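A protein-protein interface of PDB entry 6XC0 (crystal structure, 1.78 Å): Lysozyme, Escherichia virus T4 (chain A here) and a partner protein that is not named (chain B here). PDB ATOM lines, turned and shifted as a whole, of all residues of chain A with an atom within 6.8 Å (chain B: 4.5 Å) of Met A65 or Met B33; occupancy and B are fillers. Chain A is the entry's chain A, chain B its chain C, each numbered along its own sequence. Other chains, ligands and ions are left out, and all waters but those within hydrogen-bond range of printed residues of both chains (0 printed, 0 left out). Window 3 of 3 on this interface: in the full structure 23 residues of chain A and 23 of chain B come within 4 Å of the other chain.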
ATOM      1  N   LEU A  13      13.663  -0.817 -19.824  1.00  0.00           N
ATOM      2  CA  LEU A  13      12.728  -0.521 -20.913  1.00  0.00           C
ATOM      3  C   LEU A  13      13.162  -1.354 -22.114  1.00  0.00           C
ATOM      4  O   LEU A  13      14.236  -1.097 -22.653  1.00  0.00           O
ATOM      5  CB  LEU A  13      12.738   0.977 -21.258  1.00  0.00           C
ATOM      6  CG  LEU A  13      11.828   1.363 -22.446  1.00  0.00           C
ATOM      7  CD1 LEU A  13      10.404   0.911 -22.177  1.00  0.00           C
ATOM      8  CD2 LEU A  13      11.867   2.829 -22.654  1.00  0.00           C
ATOM      9  N   ARG A  14      12.354  -2.337 -22.509  1.00  0.00           N
ATOM     10  CA  ARG A  14      12.646  -3.192 -23.657  1.00  0.00           C
ATOM     11  C   ARG A  14      11.532  -3.114 -24.677  1.00  0.00           C
ATOM     12  O   ARG A  14      10.354  -3.163 -24.316  1.00  0.00           O
ATOM     13  CB  ARG A  14      12.834  -4.664 -23.216  1.00  0.00           C
ATOM     14  CG  ARG A  14      14.214  -4.892 -22.579  1.00  0.00           C
ATOM     15  CD  ARG A  14      15.253  -4.998 -23.682  1.00  0.00           C
ATOM     16  NE  ARG A  14      15.094  -6.237 -24.442  1.00  0.00           N
ATOM     17  CZ  ARG A  14      15.943  -6.670 -25.390  1.00  0.00           C
ATOM     18  NH1 ARG A  14      17.020  -5.972 -25.723  1.00  0.00           N
ATOM     19  NH2 ARG A  14      15.700  -7.789 -26.015  1.00  0.00           N
ATOM     20  N   LEU A  15      11.891  -3.032 -25.964  1.00  0.00           N
ATOM     21  CA  LEU A  15      10.889  -3.119 -27.012  1.00  0.00           C
ATOM     22  C   LEU A  15      10.893  -4.500 -27.678  1.00  0.00           C
ATOM     23  O   LEU A  15      10.106  -4.740 -28.600  1.00  0.00           O
ATOM     24  CB  LEU A  15      11.109  -2.022 -28.072  1.00  0.00           C
ATOM     25  CG  LEU A  15      11.113  -0.608 -27.484  1.00  0.00           C
ATOM     26  CD1 LEU A  15      11.325   0.408 -28.579  1.00  0.00           C
ATOM     27  CD2 LEU A  15       9.831  -0.354 -26.702  1.00  0.00           C
ATOM     28  N   LYS A  16      11.795  -5.399 -27.236  1.00  0.00           N
ATOM     29  CA  LYS A  16      11.924  -6.775 -27.704  1.00  0.00           C
ATOM     30  C   LYS A  16      11.939  -7.672 -26.474  1.00  0.00           C
ATOM     31  O   LYS A  16      12.487  -7.293 -25.429  1.00  0.00           O
ATOM     32  CB  LYS A  16      13.212  -6.965 -28.508  1.00  0.00           C
ATOM     33  CG  LYS A  16      13.660  -8.417 -28.698  1.00  0.00           C
ATOM     34  CD  LYS A  16      14.811  -8.591 -29.725  1.00  0.00           C
ATOM     35  CE  LYS A  16      14.322  -8.395 -31.202  1.00  0.00           C
ATOM     36  NZ  LYS A  16      13.575  -7.122 -31.487  1.00  0.00           N
ATOM     37  N   VAL A  17      11.317  -8.849 -26.615  1.00  0.00           N
ATOM     38  CA  VAL A  17      11.255  -9.818 -25.523  1.00  0.00           C
ATOM     39  C   VAL A  17      12.635 -10.104 -24.925  1.00  0.00           C
ATOM     40  O   VAL A  17      13.633 -10.212 -25.639  1.00  0.00           O
ATOM     41  CB  VAL A  17      10.613 -11.107 -26.052  1.00  0.00           C
ATOM     42  CG1 VAL A  17      10.633 -12.209 -24.950  1.00  0.00           C
ATOM     43  CG2 VAL A  17       9.159 -10.794 -26.444  1.00  0.00           C
ATOM     44  N   ILE A  27       8.779  -8.032 -21.420  1.00  0.00           N
ATOM     45  CA  ILE A  27       8.972  -6.953 -22.388  1.00  0.00           C
ATOM     46  C   ILE A  27       8.531  -5.619 -21.781  1.00  0.00           C
ATOM     47  O   ILE A  27       8.017  -5.571 -20.661  1.00  0.00           O
ATOM     48  CB  ILE A  27       8.222  -7.262 -23.694  1.00  0.00           C
ATOM     49  CG1 ILE A  27       8.721  -6.408 -24.865  1.00  0.00           C
ATOM     50  CG2 ILE A  27       6.690  -7.052 -23.513  1.00  0.00           C
ATOM     51  CD1 ILE A  27       8.292  -7.011 -26.184  1.00  0.00           C
ATOM     52  N   ILE A  63       7.571  -4.740 -29.787  1.00  0.00           N
ATOM     53  CA  ILE A  63       6.488  -3.771 -29.663  1.00  0.00           C
ATOM     54  C   ILE A  63       7.048  -2.380 -29.914  1.00  0.00           C
ATOM     55  O   ILE A  63       8.271  -2.158 -29.987  1.00  0.00           O
ATOM     56  CB  ILE A  63       5.786  -3.844 -28.291  1.00  0.00           C
ATOM     57  CG1 ILE A  63       6.790  -3.623 -27.157  1.00  0.00           C
ATOM     58  CG2 ILE A  63       5.032  -5.179 -28.133  1.00  0.00           C
ATOM     59  CD1 ILE A  63       6.130  -3.686 -25.825  1.00  0.00           C
ATOM     60  N   THR A  64       6.135  -1.433 -30.090  1.00  0.00           N
ATOM     61  CA  THR A  64       6.530  -0.039 -30.212  1.00  0.00           C
ATOM     62  C   THR A  64       6.595   0.598 -28.826  1.00  0.00           C
ATOM     63  O   THR A  64       6.084   0.067 -27.849  1.00  0.00           O
ATOM     64  CB  THR A  64       5.516   0.742 -31.048  1.00  0.00           C
ATOM     65  OG1 THR A  64       4.276   0.748 -30.318  1.00  0.00           O
ATOM     66  CG2 THR A  64       5.332   0.126 -32.468  1.00  0.00           C
ATOM     67  N   MET A  65       7.181   1.787 -28.767  1.00  0.00           N
ATOM     68  CA  MET A  65       7.245   2.511 -27.507  1.00  0.00           C
ATOM     69  C   MET A  65       5.845   2.853 -27.007  1.00  0.00           C
ATOM     70  O   MET A  65       5.573   2.793 -25.799  1.00  0.00           O
ATOM     71  CB  MET A  65       8.107   3.764 -27.666  1.00  0.00           C
ATOM     72  CG  MET A  65       8.211   4.530 -26.402  1.00  0.00           C
ATOM     73  SD  MET A  65       9.333   3.705 -25.216  1.00  0.00           S
ATOM     74  CE  MET A  65      10.887   3.996 -26.044  1.00  0.00           C
ATOM     75  N   GLU A  66       4.925   3.169 -27.921  1.00  0.00           N
ATOM     76  CA  GLU A  66       3.568   3.497 -27.487  1.00  0.00           C
ATOM     77  C   GLU A  66       2.895   2.278 -26.877  1.00  0.00           C
ATOM     78  O   GLU A  66       2.187   2.393 -25.869  1.00  0.00           O
ATOM     79  CB  GLU A  66       2.741   4.031 -28.671  1.00  0.00           C
ATOM     80  CG  GLU A  66       1.384   4.567 -28.234  1.00  0.00           C
ATOM     81  CD  GLU A  66       0.522   5.095 -29.376  1.00  0.00           C
ATOM     82  OE1 GLU A  66       1.046   5.308 -30.494  1.00  0.00           O
ATOM     83  OE2 GLU A  66      -0.691   5.306 -29.150  1.00  0.00           O
ATOM     84  N   GLU A  67       3.144   1.096 -27.445  1.00  0.00           N
ATOM     85  CA  GLU A  67       2.581  -0.134 -26.890  1.00  0.00           C
ATOM     86  C   GLU A  67       3.184  -0.458 -25.530  1.00  0.00           C
ATOM     87  O   GLU A  67       2.485  -0.933 -24.638  1.00  0.00           O
ATOM     88  CB  GLU A  67       2.788  -1.301 -27.859  1.00  0.00           C
ATOM     89  CG  GLU A  67       1.829  -1.188 -29.091  1.00  0.00           C
ATOM     90  CD  GLU A  67       2.254  -1.947 -30.322  1.00  0.00           C
ATOM     91  OE1 GLU A  67       3.410  -2.444 -30.410  1.00  0.00           O
ATOM     92  OE2 GLU A  67       1.400  -2.028 -31.236  1.00  0.00           O
ATOM     93  N   ALA A  68       4.485  -0.236 -25.365  1.00  0.00           N
ATOM     94  CA  ALA A  68       5.108  -0.503 -24.073  1.00  0.00           C
ATOM     95  C   ALA A  68       4.488   0.358 -22.967  1.00  0.00           C
ATOM     96  O   ALA A  68       4.286  -0.119 -21.828  1.00  0.00           O
ATOM     97  CB  ALA A  68       6.622  -0.266 -24.185  1.00  0.00           C
ATOM     98  N   THR A  69       4.187   1.624 -23.287  1.00  0.00           N
ATOM     99  CA  THR A  69       3.559   2.542 -22.345  1.00  0.00           C
ATOM    100  C   THR A  69       2.156   2.089 -21.990  1.00  0.00           C
ATOM    101  O   THR A  69       1.756   2.136 -20.814  1.00  0.00           O
ATOM    102  CB  THR A  69       3.511   3.960 -22.935  1.00  0.00           C
ATOM    103  OG1 THR A  69       4.852   4.448 -23.080  1.00  0.00           O
ATOM    104  CG2 THR A  69       2.717   4.881 -22.033  1.00  0.00           C
ATOM    105  N   THR A  70       1.390   1.671 -22.993  1.00  0.00           N
ATOM    106  CA  THR A  70       0.035   1.164 -22.772  1.00  0.00           C
ATOM    107  C   THR A  70       0.029  -0.084 -21.897  1.00  0.00           C
ATOM    108  O   THR A  70      -0.797  -0.194 -20.982  1.00  0.00           O
ATOM    109  CB  THR A  70      -0.646   0.854 -24.104  1.00  0.00           C
ATOM    110  OG1 THR A  70      -0.762   2.053 -24.874  1.00  0.00           O
ATOM    111  CG2 THR A  70      -2.048   0.292 -23.861  1.00  0.00           C
ATOM    112  N   CYS B  29      21.179   3.490 -26.507  1.00  0.00           N
ATOM    113  CA  CYS B  29      19.797   3.573 -26.052  1.00  0.00           C
ATOM    114  C   CYS B  29      18.905   2.620 -26.849  1.00  0.00           C
ATOM    115  O   CYS B  29      18.419   1.624 -26.313  1.00  0.00           O
ATOM    116  CB  CYS B  29      19.297   5.019 -26.158  1.00  0.00           C
ATOM    117  SG  CYS B  29      17.534   5.215 -25.797  1.00  0.00           S
ATOM    118  N   GLU B  30      18.718   2.901 -28.139  1.00  0.00           N
ATOM    119  CA  GLU B  30      17.798   2.116 -28.971  1.00  0.00           C
ATOM    120  C   GLU B  30      18.296   0.685 -29.172  1.00  0.00           C
ATOM    121  O   GLU B  30      17.503  -0.263 -29.177  1.00  0.00           O
ATOM    122  CB  GLU B  30      17.562   2.831 -30.309  1.00  0.00           C
ATOM    123  CG  GLU B  30      16.794   4.113 -30.089  1.00  0.00           C
ATOM    124  CD  GLU B  30      16.644   4.950 -31.322  1.00  0.00           C
ATOM    125  OE1 GLU B  30      17.108   4.516 -32.410  1.00  0.00           O
ATOM    126  OE2 GLU B  30      16.052   6.048 -31.197  1.00  0.00           O
ATOM    127  N   TRP B  31      19.604   0.497 -29.283  1.00  0.00           N
ATOM    128  CA  TRP B  31      20.124  -0.853 -29.457  1.00  0.00           C
ATOM    129  C   TRP B  31      19.821  -1.693 -28.227  1.00  0.00           C
ATOM    130  O   TRP B  31      19.448  -2.868 -28.338  1.00  0.00           O
ATOM    131  CB  TRP B  31      21.636  -0.795 -29.711  1.00  0.00           C
ATOM    132  CG  TRP B  31      22.325  -2.135 -29.728  1.00  0.00           C
ATOM    133  CD1 TRP B  31      22.452  -2.984 -30.798  1.00  0.00           C
ATOM    134  CD2 TRP B  31      23.021  -2.770 -28.630  1.00  0.00           C
ATOM    135  NE1 TRP B  31      23.155  -4.106 -30.423  1.00  0.00           N
ATOM    136  CE2 TRP B  31      23.514  -3.997 -29.102  1.00  0.00           C
ATOM    137  CE3 TRP B  31      23.273  -2.404 -27.301  1.00  0.00           C
ATOM    138  CZ2 TRP B  31      24.258  -4.885 -28.285  1.00  0.00           C
ATOM    139  CZ3 TRP B  31      24.017  -3.273 -26.494  1.00  0.00           C
ATOM    140  CH2 TRP B  31      24.497  -4.501 -26.995  1.00  0.00           C
ATOM    141  N   SER B  32      19.924  -1.076 -27.051  1.00  0.00           N
ATOM    142  CA  SER B  32      19.729  -1.842 -25.818  1.00  0.00           C
ATOM    143  C   SER B  32      18.264  -2.216 -25.659  1.00  0.00           C
ATOM    144  O   SER B  32      17.935  -3.194 -24.967  1.00  0.00           O
ATOM    145  CB  SER B  32      20.225  -1.046 -24.614  1.00  0.00           C
ATOM    146  OG  SER B  32      19.326  -0.007 -24.311  1.00  0.00           O
ATOM    147  N   MET B  33      17.374  -1.409 -26.238  1.00  0.00           N
ATOM    148  CA  MET B  33      15.946  -1.722 -26.169  1.00  0.00           C
ATOM    149  C   MET B  33      15.533  -2.835 -27.114  1.00  0.00           C
ATOM    150  O   MET B  33      14.455  -3.433 -26.925  1.00  0.00           O
ATOM    151  CB  MET B  33      15.120  -0.478 -26.486  1.00  0.00           C
ATOM    152  CG  MET B  33      15.239   0.598 -25.401  1.00  0.00           C
ATOM    153  SD  MET B  33      14.043   1.908 -25.700  1.00  0.00           S
ATOM    154  CE  MET B  33      14.583   2.494 -27.309  1.00  0.00           C
ATOM    155  N   THR B  34      16.324  -3.097 -28.172  1.00  0.00           N
ATOM    156  CA  THR B  34      15.883  -3.934 -29.265  1.00  0.00           C
ATOM    157  C   THR B  34      16.780  -5.121 -29.578  1.00  0.00           C
ATOM    158  O   THR B  34      16.307  -6.053 -30.218  1.00  0.00           O
ATOM    159  CB  THR B  34      15.742  -3.101 -30.559  1.00  0.00           C
ATOM    160  OG1 THR B  34      17.013  -2.498 -30.889  1.00  0.00           O
ATOM    161  CG2 THR B  34      14.729  -1.997 -30.338  1.00  0.00           C
ATOM    162  N   ALA B  35      18.052  -5.105 -29.194  1.00  0.00           N
ATOM    163  CA  ALA B  35      18.941  -6.177 -29.604  1.00  0.00           C
ATOM    164  C   ALA B  35      18.714  -7.423 -28.750  1.00  0.00           C
ATOM    165  O   ALA B  35      18.137  -7.343 -27.666  1.00  0.00           O
ATOM    166  CB  ALA B  35      20.391  -5.724 -29.484  1.00  0.00           C
ATOM    167  N   ASN B  76      19.442  -1.062 -18.430  1.00  0.00           N
ATOM    168  CA  ASN B  76      19.637  -0.442 -19.734  1.00  0.00           C
ATOM    169  C   ASN B  76      19.142   1.002 -19.707  1.00  0.00           C
ATOM    170  O   ASN B  76      19.747   1.882 -20.334  1.00  0.00           O
ATOM    171  CB  ASN B  76      18.965  -1.254 -20.855  1.00  0.00           C
ATOM    172  CG  ASN B  76      17.442  -0.980 -20.991  1.00  0.00           C
ATOM    173  OD1 ASN B  76      16.675  -1.083 -20.049  1.00  0.00           O
ATOM    174  ND2 ASN B  76      17.027  -0.620 -22.194  1.00  0.00           N
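O of Leu A13 is in hydrogen-bond range of ND2 of Asn B76, 2.9 Å away. The backbone carbonyl oxygen (O) of Ser B32 is in hydrogen-bond range of the guanidinium group (NH1) of Arg A14 (3.0 Å). NH1 of Arg A14 is in hydrogen-bond range of O of Ala B35 (2.6 Å). N of Leu A15 is in hydrogen-bond range of O of Met B33 (2.8 Å). The backbone NH (N) of Lys A16 is in hydrogen-bond range of the backbone carbonyl oxygen (O) of Met B33. NZ of Lys A16 sits close to O of Thr B34.
The guanidinium group (NH2) of Arg A14 sits at hydrogen-bond distance from the backbone carbonyl oxygen (O) of Val A17 (3.2 Å). N of Ile A63 sits at hydrogen-bond distance from O of Leu A15 (2.8 Å). O of Met A65 is in hydrogen-bond range of OG1 of Thr A69. O of Cys B29 sits at hydrogen-bond distance from OG of Ser B32, at 2.7 Å. The backbone carbonyl oxygen (O) of Glu B30 is in hydrogen-bond range of the side-chain hydroxyl (OG1) of Thr B34 (2.9 Å). OG of Ser B32 sits at hydrogen-bond distance from ND2 of Asn B76, at 3.2 Å.
Met B33 touches Leu A13 (CG to O, 3.4 Å). Arg A14 touches Met B33. NH1 of Arg A14 touches N of Thr B34, at 3.8 Å. Met A65 touches Met B33.
Printed residues of chain B within 4 Å of Leu A15: Met B33. Ile A63 touches none of the printed residues of chain B. Met A65 touches just one residue of chain B: Met B33 (3.8 Å). Glu A66 touches none of the printed residues of chain B. Met B33 touches just these residues of chain A: Leu A13 (3.4 Å), Arg A14 (3.7 Å), Leu A15 (2.8 Å), Lys A16 (3.3 Å) and Met A65 (3.8 Å). Of the printed residues of chain A, Thr B34 touches Arg A14 and Lys A16. The nearest printed residue of chain B that does not touch Met A65 is Cys B29 (6.8 Å). The nearest printed residue of chain B that does not touch Leu A13 is Ser B32 (4.8 Å).
Hydrophobic or aromatic side chains of chain A that line the printed part of chain B: Leu A13, Leu A15 and Met A65. Hydrophobic or aromatic side chains of chain B that line the printed part of chain A: Met B33. Among the printed residues, 10 pairs touch across the chains. Among the printed residues, no Asp or Glu carboxylate lies within 4 Å of a Lys or Arg side-chain nitrogen of the other chain.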
